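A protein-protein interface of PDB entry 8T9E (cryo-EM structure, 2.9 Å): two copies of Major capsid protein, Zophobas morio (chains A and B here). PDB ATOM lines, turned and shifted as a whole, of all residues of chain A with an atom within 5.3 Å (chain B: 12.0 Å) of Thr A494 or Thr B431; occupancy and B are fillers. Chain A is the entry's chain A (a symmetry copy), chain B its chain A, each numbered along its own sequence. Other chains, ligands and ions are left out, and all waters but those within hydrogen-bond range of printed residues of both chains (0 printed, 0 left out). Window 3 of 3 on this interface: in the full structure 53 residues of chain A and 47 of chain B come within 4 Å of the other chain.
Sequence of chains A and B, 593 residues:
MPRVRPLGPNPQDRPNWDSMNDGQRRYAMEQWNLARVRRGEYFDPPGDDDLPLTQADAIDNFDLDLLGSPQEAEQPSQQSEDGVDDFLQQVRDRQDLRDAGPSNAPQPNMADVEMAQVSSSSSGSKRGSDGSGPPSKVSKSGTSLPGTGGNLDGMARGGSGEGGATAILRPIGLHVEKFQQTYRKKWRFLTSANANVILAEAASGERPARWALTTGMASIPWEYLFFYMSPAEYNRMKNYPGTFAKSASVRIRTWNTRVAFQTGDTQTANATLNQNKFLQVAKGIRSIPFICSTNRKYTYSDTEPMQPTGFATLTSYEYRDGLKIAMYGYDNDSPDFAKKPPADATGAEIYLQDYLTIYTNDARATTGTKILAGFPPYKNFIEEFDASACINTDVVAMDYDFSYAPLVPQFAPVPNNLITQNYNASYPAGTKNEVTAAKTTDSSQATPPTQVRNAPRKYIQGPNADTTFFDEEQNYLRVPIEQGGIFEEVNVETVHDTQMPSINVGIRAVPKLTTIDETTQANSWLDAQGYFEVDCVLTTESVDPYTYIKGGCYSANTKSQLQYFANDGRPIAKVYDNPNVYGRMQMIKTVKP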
ATOM      1  N   ASN A 433     -30.374 -12.370  -2.862  1.00  0.00           N
ATOM      2  CA  ASN A 433     -29.942 -12.347  -1.475  1.00  0.00           C
ATOM      3  C   ASN A 433     -30.942 -11.543  -0.661  1.00  0.00           C
ATOM      4  O   ASN A 433     -31.251 -10.399  -1.002  1.00  0.00           O
ATOM      5  CB  ASN A 433     -28.549 -11.734  -1.339  1.00  0.00           C
ATOM      6  CG  ASN A 433     -27.502 -12.491  -2.111  1.00  0.00           C
ATOM      7  OD1 ASN A 433     -26.731 -11.902  -2.863  1.00  0.00           O
ATOM      8  ND2 ASN A 433     -27.462 -13.802  -1.929  1.00  0.00           N
ATOM      9  N   GLU A 434     -31.456 -12.148   0.408  1.00  0.00           N
ATOM     10  CA  GLU A 434     -32.313 -11.430   1.339  1.00  0.00           C
ATOM     11  C   GLU A 434     -31.833 -11.589   2.775  1.00  0.00           C
ATOM     12  O   GLU A 434     -32.582 -11.306   3.713  1.00  0.00           O
ATOM     13  CB  GLU A 434     -33.770 -11.865   1.186  1.00  0.00           C
ATOM     14  CG  GLU A 434     -33.995 -13.354   1.171  1.00  0.00           C
ATOM     15  CD  GLU A 434     -35.301 -13.714   0.499  1.00  0.00           C
ATOM     16  OE1 GLU A 434     -35.325 -13.789  -0.747  1.00  0.00           O
ATOM     17  OE2 GLU A 434     -36.308 -13.910   1.209  1.00  0.00           O
ATOM     18  N   VAL A 435     -30.593 -12.035   2.955  1.00  0.00           N
ATOM     19  CA  VAL A 435     -29.877 -11.930   4.217  1.00  0.00           C
ATOM     20  C   VAL A 435     -28.578 -11.193   3.935  1.00  0.00           C
ATOM     21  O   VAL A 435     -27.801 -11.606   3.066  1.00  0.00           O
ATOM     22  CB  VAL A 435     -29.603 -13.307   4.846  1.00  0.00           C
ATOM     23  CG1 VAL A 435     -28.674 -13.167   6.029  1.00  0.00           C
ATOM     24  CG2 VAL A 435     -30.904 -13.949   5.274  1.00  0.00           C
ATOM     25  N   THR A 436     -28.348 -10.100   4.652  1.00  0.00           N
ATOM     26  CA  THR A 436     -27.201  -9.250   4.377  1.00  0.00           C
ATOM     27  C   THR A 436     -25.909  -9.915   4.833  1.00  0.00           C
ATOM     28  O   THR A 436     -25.902 -10.782   5.711  1.00  0.00           O
ATOM     29  CB  THR A 436     -27.364  -7.899   5.069  1.00  0.00           C
ATOM     30  OG1 THR A 436     -27.424  -8.093   6.486  1.00  0.00           O
ATOM     31  CG2 THR A 436     -28.642  -7.228   4.611  1.00  0.00           C
ATOM     32  N   ARG A 453     -21.863 -14.196   5.081  1.00  0.00           N
ATOM     33  CA  ARG A 453     -23.300 -14.066   5.237  1.00  0.00           C
ATOM     34  C   ARG A 453     -23.731 -14.647   6.581  1.00  0.00           C
ATOM     35  O   ARG A 453     -23.010 -15.427   7.207  1.00  0.00           O
ATOM     36  CB  ARG A 453     -24.015 -14.766   4.079  1.00  0.00           C
ATOM     37  CG  ARG A 453     -25.520 -14.593   4.025  1.00  0.00           C
ATOM     38  CD  ARG A 453     -26.038 -14.702   2.610  1.00  0.00           C
ATOM     39  NE  ARG A 453     -26.025 -13.418   1.924  1.00  0.00           N
ATOM     40  CZ  ARG A 453     -25.213 -13.109   0.924  1.00  0.00           C
ATOM     41  NH1 ARG A 453     -24.330 -13.974   0.460  1.00  0.00           N
ATOM     42  NH2 ARG A 453     -25.293 -11.903   0.374  1.00  0.00           N
ATOM     43  N   VAL A 492     -37.931  -9.068   1.708  1.00  0.00           N
ATOM     44  CA  VAL A 492     -37.176  -9.169   0.462  1.00  0.00           C
ATOM     45  C   VAL A 492     -36.591  -7.843   0.006  1.00  0.00           C
ATOM     46  O   VAL A 492     -36.108  -7.756  -1.128  1.00  0.00           O
ATOM     47  CB  VAL A 492     -38.048  -9.725  -0.679  1.00  0.00           C
ATOM     48  CG1 VAL A 492     -38.276 -11.208  -0.492  1.00  0.00           C
ATOM     49  CG2 VAL A 492     -39.369  -8.984  -0.742  1.00  0.00           C
ATOM     50  N   GLU A 493     -36.623  -6.808   0.843  1.00  0.00           N
ATOM     51  CA  GLU A 493     -36.135  -5.506   0.413  1.00  0.00           C
ATOM     52  C   GLU A 493     -34.627  -5.544   0.204  1.00  0.00           C
ATOM     53  O   GLU A 493     -33.920  -6.393   0.751  1.00  0.00           O
ATOM     54  CB  GLU A 493     -36.484  -4.421   1.432  1.00  0.00           C
ATOM     55  CG  GLU A 493     -35.795  -4.574   2.778  1.00  0.00           C
ATOM     56  CD  GLU A 493     -36.216  -3.510   3.776  1.00  0.00           C
ATOM     57  OE1 GLU A 493     -37.066  -2.664   3.427  1.00  0.00           O
ATOM     58  OE2 GLU A 493     -35.684  -3.510   4.904  1.00  0.00           O
ATOM     59  N   THR A 494     -34.138  -4.610  -0.604  1.00  0.00           N
ATOM     60  CA  THR A 494     -32.713  -4.532  -0.887  1.00  0.00           C
ATOM     61  C   THR A 494     -32.016  -3.652   0.142  1.00  0.00           C
ATOM     62  O   THR A 494     -32.491  -2.564   0.472  1.00  0.00           O
ATOM     63  CB  THR A 494     -32.485  -3.985  -2.295  1.00  0.00           C
ATOM     64  OG1 THR A 494     -33.027  -4.896  -3.255  1.00  0.00           O
ATOM     65  CG2 THR A 494     -31.003  -3.807  -2.566  1.00  0.00           C
ATOM     66  N   VAL A 495     -30.884  -4.130   0.650  1.00  0.00           N
ATOM     67  CA  VAL A 495     -30.040  -3.386   1.576  1.00  0.00           C
ATOM     68  C   VAL A 495     -28.743  -3.055   0.857  1.00  0.00           C
ATOM     69  O   VAL A 495     -28.230  -3.875   0.088  1.00  0.00           O
ATOM     70  CB  VAL A 495     -29.774  -4.188   2.862  1.00  0.00           C
ATOM     71  CG1 VAL A 495     -28.869  -3.417   3.800  1.00  0.00           C
ATOM     72  CG2 VAL A 495     -31.080  -4.533   3.549  1.00  0.00           C
ATOM     73  N   HIS A 496     -28.235  -1.845   1.070  1.00  0.00           N
ATOM     74  CA  HIS A 496     -26.966  -1.432   0.493  1.00  0.00           C
ATOM     75  C   HIS A 496     -26.210  -0.556   1.481  1.00  0.00           C
ATOM     76  O   HIS A 496     -26.794   0.076   2.362  1.00  0.00           O
ATOM     77  CB  HIS A 496     -27.163  -0.691  -0.837  1.00  0.00           C
ATOM     78  CG  HIS A 496     -27.918   0.595  -0.710  1.00  0.00           C
ATOM     79  ND1 HIS A 496     -29.294   0.655  -0.724  1.00  0.00           N
ATOM     80  CD2 HIS A 496     -27.488   1.872  -0.577  1.00  0.00           C
ATOM     81  CE1 HIS A 496     -29.680   1.912  -0.599  1.00  0.00           C
ATOM     82  NE2 HIS A 496     -28.602   2.671  -0.508  1.00  0.00           N
ATOM     83  N   TYR B 427     -17.028  -3.725   6.876  1.00  0.00           N
ATOM     84  CA  TYR B 427     -18.083  -2.756   6.635  1.00  0.00           C
ATOM     85  C   TYR B 427     -19.269  -3.496   6.046  1.00  0.00           C
ATOM     86  O   TYR B 427     -19.090  -4.542   5.414  1.00  0.00           O
ATOM     87  CB  TYR B 427     -17.629  -1.623   5.702  1.00  0.00           C
ATOM     88  CG  TYR B 427     -16.860  -2.064   4.485  1.00  0.00           C
ATOM     89  CD1 TYR B 427     -17.517  -2.510   3.352  1.00  0.00           C
ATOM     90  CD2 TYR B 427     -15.476  -2.014   4.463  1.00  0.00           C
ATOM     91  CE1 TYR B 427     -16.819  -2.905   2.237  1.00  0.00           C
ATOM     92  CE2 TYR B 427     -14.769  -2.407   3.351  1.00  0.00           C
ATOM     93  CZ  TYR B 427     -15.445  -2.850   2.241  1.00  0.00           C
ATOM     94  OH  TYR B 427     -14.750  -3.241   1.124  1.00  0.00           O
ATOM     95  N   PRO B 428     -20.479  -2.998   6.244  1.00  0.00           N
ATOM     96  CA  PRO B 428     -21.655  -3.783   5.863  1.00  0.00           C
ATOM     97  C   PRO B 428     -21.916  -3.816   4.370  1.00  0.00           C
ATOM     98  O   PRO B 428     -22.348  -2.818   3.788  1.00  0.00           O
ATOM     99  CB  PRO B 428     -22.793  -3.075   6.602  1.00  0.00           C
ATOM    100  CG  PRO B 428     -22.337  -1.679   6.723  1.00  0.00           C
ATOM    101  CD  PRO B 428     -20.855  -1.746   6.923  1.00  0.00           C
ATOM    102  N   ALA B 429     -21.656  -4.952   3.736  1.00  0.00           N
ATOM    103  CA  ALA B 429     -22.252  -5.206   2.436  1.00  0.00           C
ATOM    104  C   ALA B 429     -23.756  -5.354   2.610  1.00  0.00           C
ATOM    105  O   ALA B 429     -24.237  -5.779   3.662  1.00  0.00           O
ATOM    106  CB  ALA B 429     -21.660  -6.463   1.802  1.00  0.00           C
ATOM    107  N   GLY B 430     -24.508  -4.970   1.593  1.00  0.00           N
ATOM    108  CA  GLY B 430     -25.942  -5.109   1.709  1.00  0.00           C
ATOM    109  C   GLY B 430     -26.384  -6.501   1.328  1.00  0.00           C
ATOM    110  O   GLY B 430     -25.795  -7.490   1.768  1.00  0.00           O
ATOM    111  N   THR B 431     -27.429  -6.592   0.516  1.00  0.00           N
ATOM    112  CA  THR B 431     -27.762  -7.844  -0.140  1.00  0.00           C
ATOM    113  C   THR B 431     -27.001  -8.020  -1.444  1.00  0.00           C
ATOM    114  O   THR B 431     -27.207  -9.017  -2.141  1.00  0.00           O
ATOM    115  CB  THR B 431     -29.267  -7.921  -0.396  1.00  0.00           C
ATOM    116  OG1 THR B 431     -29.671  -6.810  -1.203  1.00  0.00           O
ATOM    117  CG2 THR B 431     -30.024  -7.882   0.917  1.00  0.00           C
ATOM    118  N   LYS B 432     -26.134  -7.072  -1.785  1.00  0.00           N
ATOM    119  CA  LYS B 432     -25.337  -7.173  -2.995  1.00  0.00           C
ATOM    120  C   LYS B 432     -24.100  -8.022  -2.744  1.00  0.00           C
ATOM    121  O   LYS B 432     -23.519  -7.996  -1.658  1.00  0.00           O
ATOM    122  CB  LYS B 432     -24.927  -5.781  -3.470  1.00  0.00           C
ATOM    123  CG  LYS B 432     -26.089  -4.917  -3.920  1.00  0.00           C
ATOM    124  CD  LYS B 432     -25.622  -3.555  -4.392  1.00  0.00           C
ATOM    125  CE  LYS B 432     -26.785  -2.732  -4.923  1.00  0.00           C
ATOM    126  NZ  LYS B 432     -27.748  -2.375  -3.843  1.00  0.00           N
ATOM    127  N   ASN B 433     -23.704  -8.787  -3.754  1.00  0.00           N
ATOM    128  CA  ASN B 433     -22.457  -9.531  -3.705  1.00  0.00           C
ATOM    129  C   ASN B 433     -21.344  -8.661  -4.266  1.00  0.00           C
ATOM    130  O   ASN B 433     -21.456  -8.141  -5.379  1.00  0.00           O
ATOM    131  CB  ASN B 433     -22.554 -10.828  -4.505  1.00  0.00           C
ATOM    132  CG  ASN B 433     -23.631 -11.748  -3.994  1.00  0.00           C
ATOM    133  OD1 ASN B 433     -24.453 -12.239  -4.762  1.00  0.00           O
ATOM    134  ND2 ASN B 433     -23.634 -11.993  -2.692  1.00  0.00           N
ATOM    135  N   GLU B 434     -20.276  -8.495  -3.489  1.00  0.00           N
ATOM    136  CA  GLU B 434     -19.092  -7.801  -3.976  1.00  0.00           C
ATOM    137  C   GLU B 434     -17.831  -8.625  -3.751  1.00  0.00           C
ATOM    138  O   GLU B 434     -16.722  -8.091  -3.824  1.00  0.00           O
ATOM    139  CB  GLU B 434     -18.974  -6.415  -3.342  1.00  0.00           C
ATOM    140  CG  GLU B 434     -19.131  -6.380  -1.846  1.00  0.00           C
ATOM    141  CD  GLU B 434     -19.539  -5.006  -1.360  1.00  0.00           C
ATOM    142  OE1 GLU B 434     -20.747  -4.696  -1.405  1.00  0.00           O
ATOM    143  OE2 GLU B 434     -18.654  -4.229  -0.947  1.00  0.00           O
ATOM    144  N   VAL B 435     -17.990  -9.917  -3.482  1.00  0.00           N
ATOM    145  CA  VAL B 435     -16.916 -10.894  -3.569  1.00  0.00           C
ATOM    146  C   VAL B 435     -17.381 -11.987  -4.518  1.00  0.00           C
ATOM    147  O   VAL B 435     -18.446 -12.579  -4.313  1.00  0.00           O
ATOM    148  CB  VAL B 435     -16.548 -11.478  -2.195  1.00  0.00           C
ATOM    149  CG1 VAL B 435     -15.593 -12.637  -2.356  1.00  0.00           C
ATOM    150  CG2 VAL B 435     -15.929 -10.406  -1.325  1.00  0.00           C
ATOM    151  N   THR B 436     -16.597 -12.243  -5.558  1.00  0.00           N
ATOM    152  CA  THR B 436     -17.006 -13.178  -6.593  1.00  0.00           C
ATOM    153  C   THR B 436     -16.938 -14.614  -6.089  1.00  0.00           C
ATOM    154  O   THR B 436     -16.205 -14.936  -5.152  1.00  0.00           O
ATOM    155  CB  THR B 436     -16.126 -13.018  -7.830  1.00  0.00           C
ATOM    156  OG1 THR B 436     -14.769 -13.321  -7.492  1.00  0.00           O
ATOM    157  CG2 THR B 436     -16.198 -11.595  -8.343  1.00  0.00           C
ATOM    158  N   GLN B 451     -21.904 -23.420  -5.704  1.00  0.00           N
ATOM    159  CA  GLN B 451     -21.279 -22.114  -5.824  1.00  0.00           C
ATOM    160  C   GLN B 451     -20.572 -21.790  -4.519  1.00  0.00           C
ATOM    161  O   GLN B 451     -21.191 -21.791  -3.453  1.00  0.00           O
ATOM    162  CB  GLN B 451     -22.307 -21.037  -6.156  1.00  0.00           C
ATOM    163  CG  GLN B 451     -21.836 -19.635  -5.874  1.00  0.00           C
ATOM    164  CD  GLN B 451     -22.888 -18.603  -6.186  1.00  0.00           C
ATOM    165  OE1 GLN B 451     -23.562 -18.681  -7.209  1.00  0.00           O
ATOM    166  NE2 GLN B 451     -23.034 -17.623  -5.307  1.00  0.00           N
ATOM    167  N   ARG B 453     -18.152 -19.100  -2.464  1.00  0.00           N
ATOM    168  CA  ARG B 453     -17.666 -17.737  -2.359  1.00  0.00           C
ATOM    169  C   ARG B 453     -16.346 -17.713  -1.592  1.00  0.00           C
ATOM    170  O   ARG B 453     -16.003 -18.654  -0.872  1.00  0.00           O
ATOM    171  CB  ARG B 453     -18.718 -16.860  -1.677  1.00  0.00           C
ATOM    172  CG  ARG B 453     -18.413 -15.376  -1.625  1.00  0.00           C
ATOM    173  CD  ARG B 453     -19.680 -14.554  -1.578  1.00  0.00           C
ATOM    174  NE  ARG B 453     -20.179 -14.245  -2.910  1.00  0.00           N
ATOM    175  CZ  ARG B 453     -21.286 -14.751  -3.434  1.00  0.00           C
ATOM    176  NH1 ARG B 453     -22.042 -15.600  -2.762  1.00  0.00           N
ATOM    177  NH2 ARG B 453     -21.642 -14.393  -4.662  1.00  0.00           N
ATOM    178  N   ASN B 491     -13.863  -3.493  -4.720  1.00  0.00           N
ATOM    179  CA  ASN B 491     -14.808  -2.450  -5.079  1.00  0.00           C
ATOM    180  C   ASN B 491     -16.203  -3.048  -5.147  1.00  0.00           C
ATOM    181  O   ASN B 491     -16.396  -4.252  -4.960  1.00  0.00           O
ATOM    182  CB  ASN B 491     -14.436  -1.801  -6.416  1.00  0.00           C
ATOM    183  CG  ASN B 491     -14.666  -0.310  -6.420  1.00  0.00           C
ATOM    184  OD1 ASN B 491     -15.180   0.254  -5.454  1.00  0.00           O
ATOM    185  ND2 ASN B 491     -14.284   0.343  -7.509  1.00  0.00           N
ATOM    186  N   VAL B 492     -17.184  -2.183  -5.417  1.00  0.00           N
ATOM    187  CA  VAL B 492     -18.568  -2.627  -5.553  1.00  0.00           C
ATOM    188  C   VAL B 492     -18.966  -2.918  -6.989  1.00  0.00           C
ATOM    189  O   VAL B 492     -20.159  -3.103  -7.259  1.00  0.00           O
ATOM    190  CB  VAL B 492     -19.549  -1.585  -4.986  1.00  0.00           C
ATOM    191  CG1 VAL B 492     -19.511  -1.594  -3.473  1.00  0.00           C
ATOM    192  CG2 VAL B 492     -19.222  -0.205  -5.521  1.00  0.00           C
ATOM    193  N   GLU B 493     -18.016  -2.958  -7.920  1.00  0.00           N
ATOM    194  CA  GLU B 493     -18.371  -3.165  -9.317  1.00  0.00           C
ATOM    195  C   GLU B 493     -18.912  -4.572  -9.528  1.00  0.00           C
ATOM    196  O   GLU B 493     -18.650  -5.489  -8.745  1.00  0.00           O
ATOM    197  CB  GLU B 493     -17.167  -2.936 -10.232  1.00  0.00           C
ATOM    198  CG  GLU B 493     -16.040  -3.938 -10.054  1.00  0.00           C
ATOM    199  CD  GLU B 493     -14.843  -3.638 -10.940  1.00  0.00           C
ATOM    200  OE1 GLU B 493     -14.883  -2.631 -11.678  1.00  0.00           O
ATOM    201  OE2 GLU B 493     -13.870  -4.419 -10.911  1.00  0.00           O
ATOM    202  N   THR B 494     -19.679  -4.736 -10.599  1.00  0.00           N
ATOM    203  CA  THR B 494     -20.259  -6.032 -10.918  1.00  0.00           C
ATOM    204  C   THR B 494     -19.305  -6.839 -11.788  1.00  0.00           C
ATOM    205  O   THR B 494     -18.739  -6.324 -12.755  1.00  0.00           O
ATOM    206  CB  THR B 494     -21.599  -5.849 -11.628  1.00  0.00           C
ATOM    207  OG1 THR B 494     -22.525  -5.211 -10.744  1.00  0.00           O
ATOM    208  CG2 THR B 494     -22.166  -7.190 -12.053  1.00  0.00           C
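O of Val A435 sits at hydrogen-bond distance from NE of Arg A453 (2.8 Å).
CA of Thr A436 touches O of Gly B430, at 3.4 Å.
Thr B431 touches Thr A436.
Thr A494 touches Thr B431.
Lys B432 touches Thr A494 (NZ to CG2, 3.8 Å).
O of Val A495 touches CA of Gly B430, 3.1 Å away.
His A496 touches Lys B432 (CB to NZ, 3.5 Å).
Of the 10 printed residues of chain A, 6 touch a printed residue of chain B.
Hydrophobic or aromatic side chains of chain A that line the printed part of chain B: Val A495 and His A496.
Asn A433 touches two residues of chain B.
Of the printed residues of chain B, Thr A436 touches Gly B430 (3.4 Å) and Thr B431 (3.998 Å).
Of the printed residues of chain B, Arg A453 touches Asn B433.
No residue of chain B comes within 4 Å of Val A492.
No residue of chain B comes within 4 Å of Glu A493.
Thr A494 touches just these residues of chain B: Thr B431 (3.6 Å) and Lys B432 (3.8 Å).
Val A495 touches just these residues of chain B: Gly B430 and Thr B431.
Printed residues of chain B within 4 Å of His A496: Lys B432.
Printed residues of chain A within 4 Å of Thr B431: Asn A433 (3.0 Å), Thr A436 (3.998 Å), Thr A494 (3.6 Å) and Val A495 (2.9 Å).
Of the printed residues of chain A, Asn B433 touches Asn A433 and Arg A453.
The nearest residue of chain B that does not touch Thr A494 is Gly B430 (6.4 Å).
Asn B433 touches its own counterpart, Asn A433.
Arg A453 touches Asn B433, but with the chains exchanged Asn A433 does not touch Arg B453 (5.8 Å).
Of the 10 pairs that touch across the chains among the printed residues, 1 has its exchanged pair printed and touching as well.
O of Thr B431 sits close to OD1 of Asn A433, 3.0 Å away.
The backbone NH of Thr B431 is in hydrogen-bond range of the backbone carbonyl oxygen of Val A495, 2.9 Å away.
The side-chain amide oxygen (OD1) of Asn B433 sits close to the side-chain amide oxygen (OD1) of Asn A433 (3.0 Å).
NH2 of Arg A453 lies close to ND2 of Asn B433 (3.5 Å).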
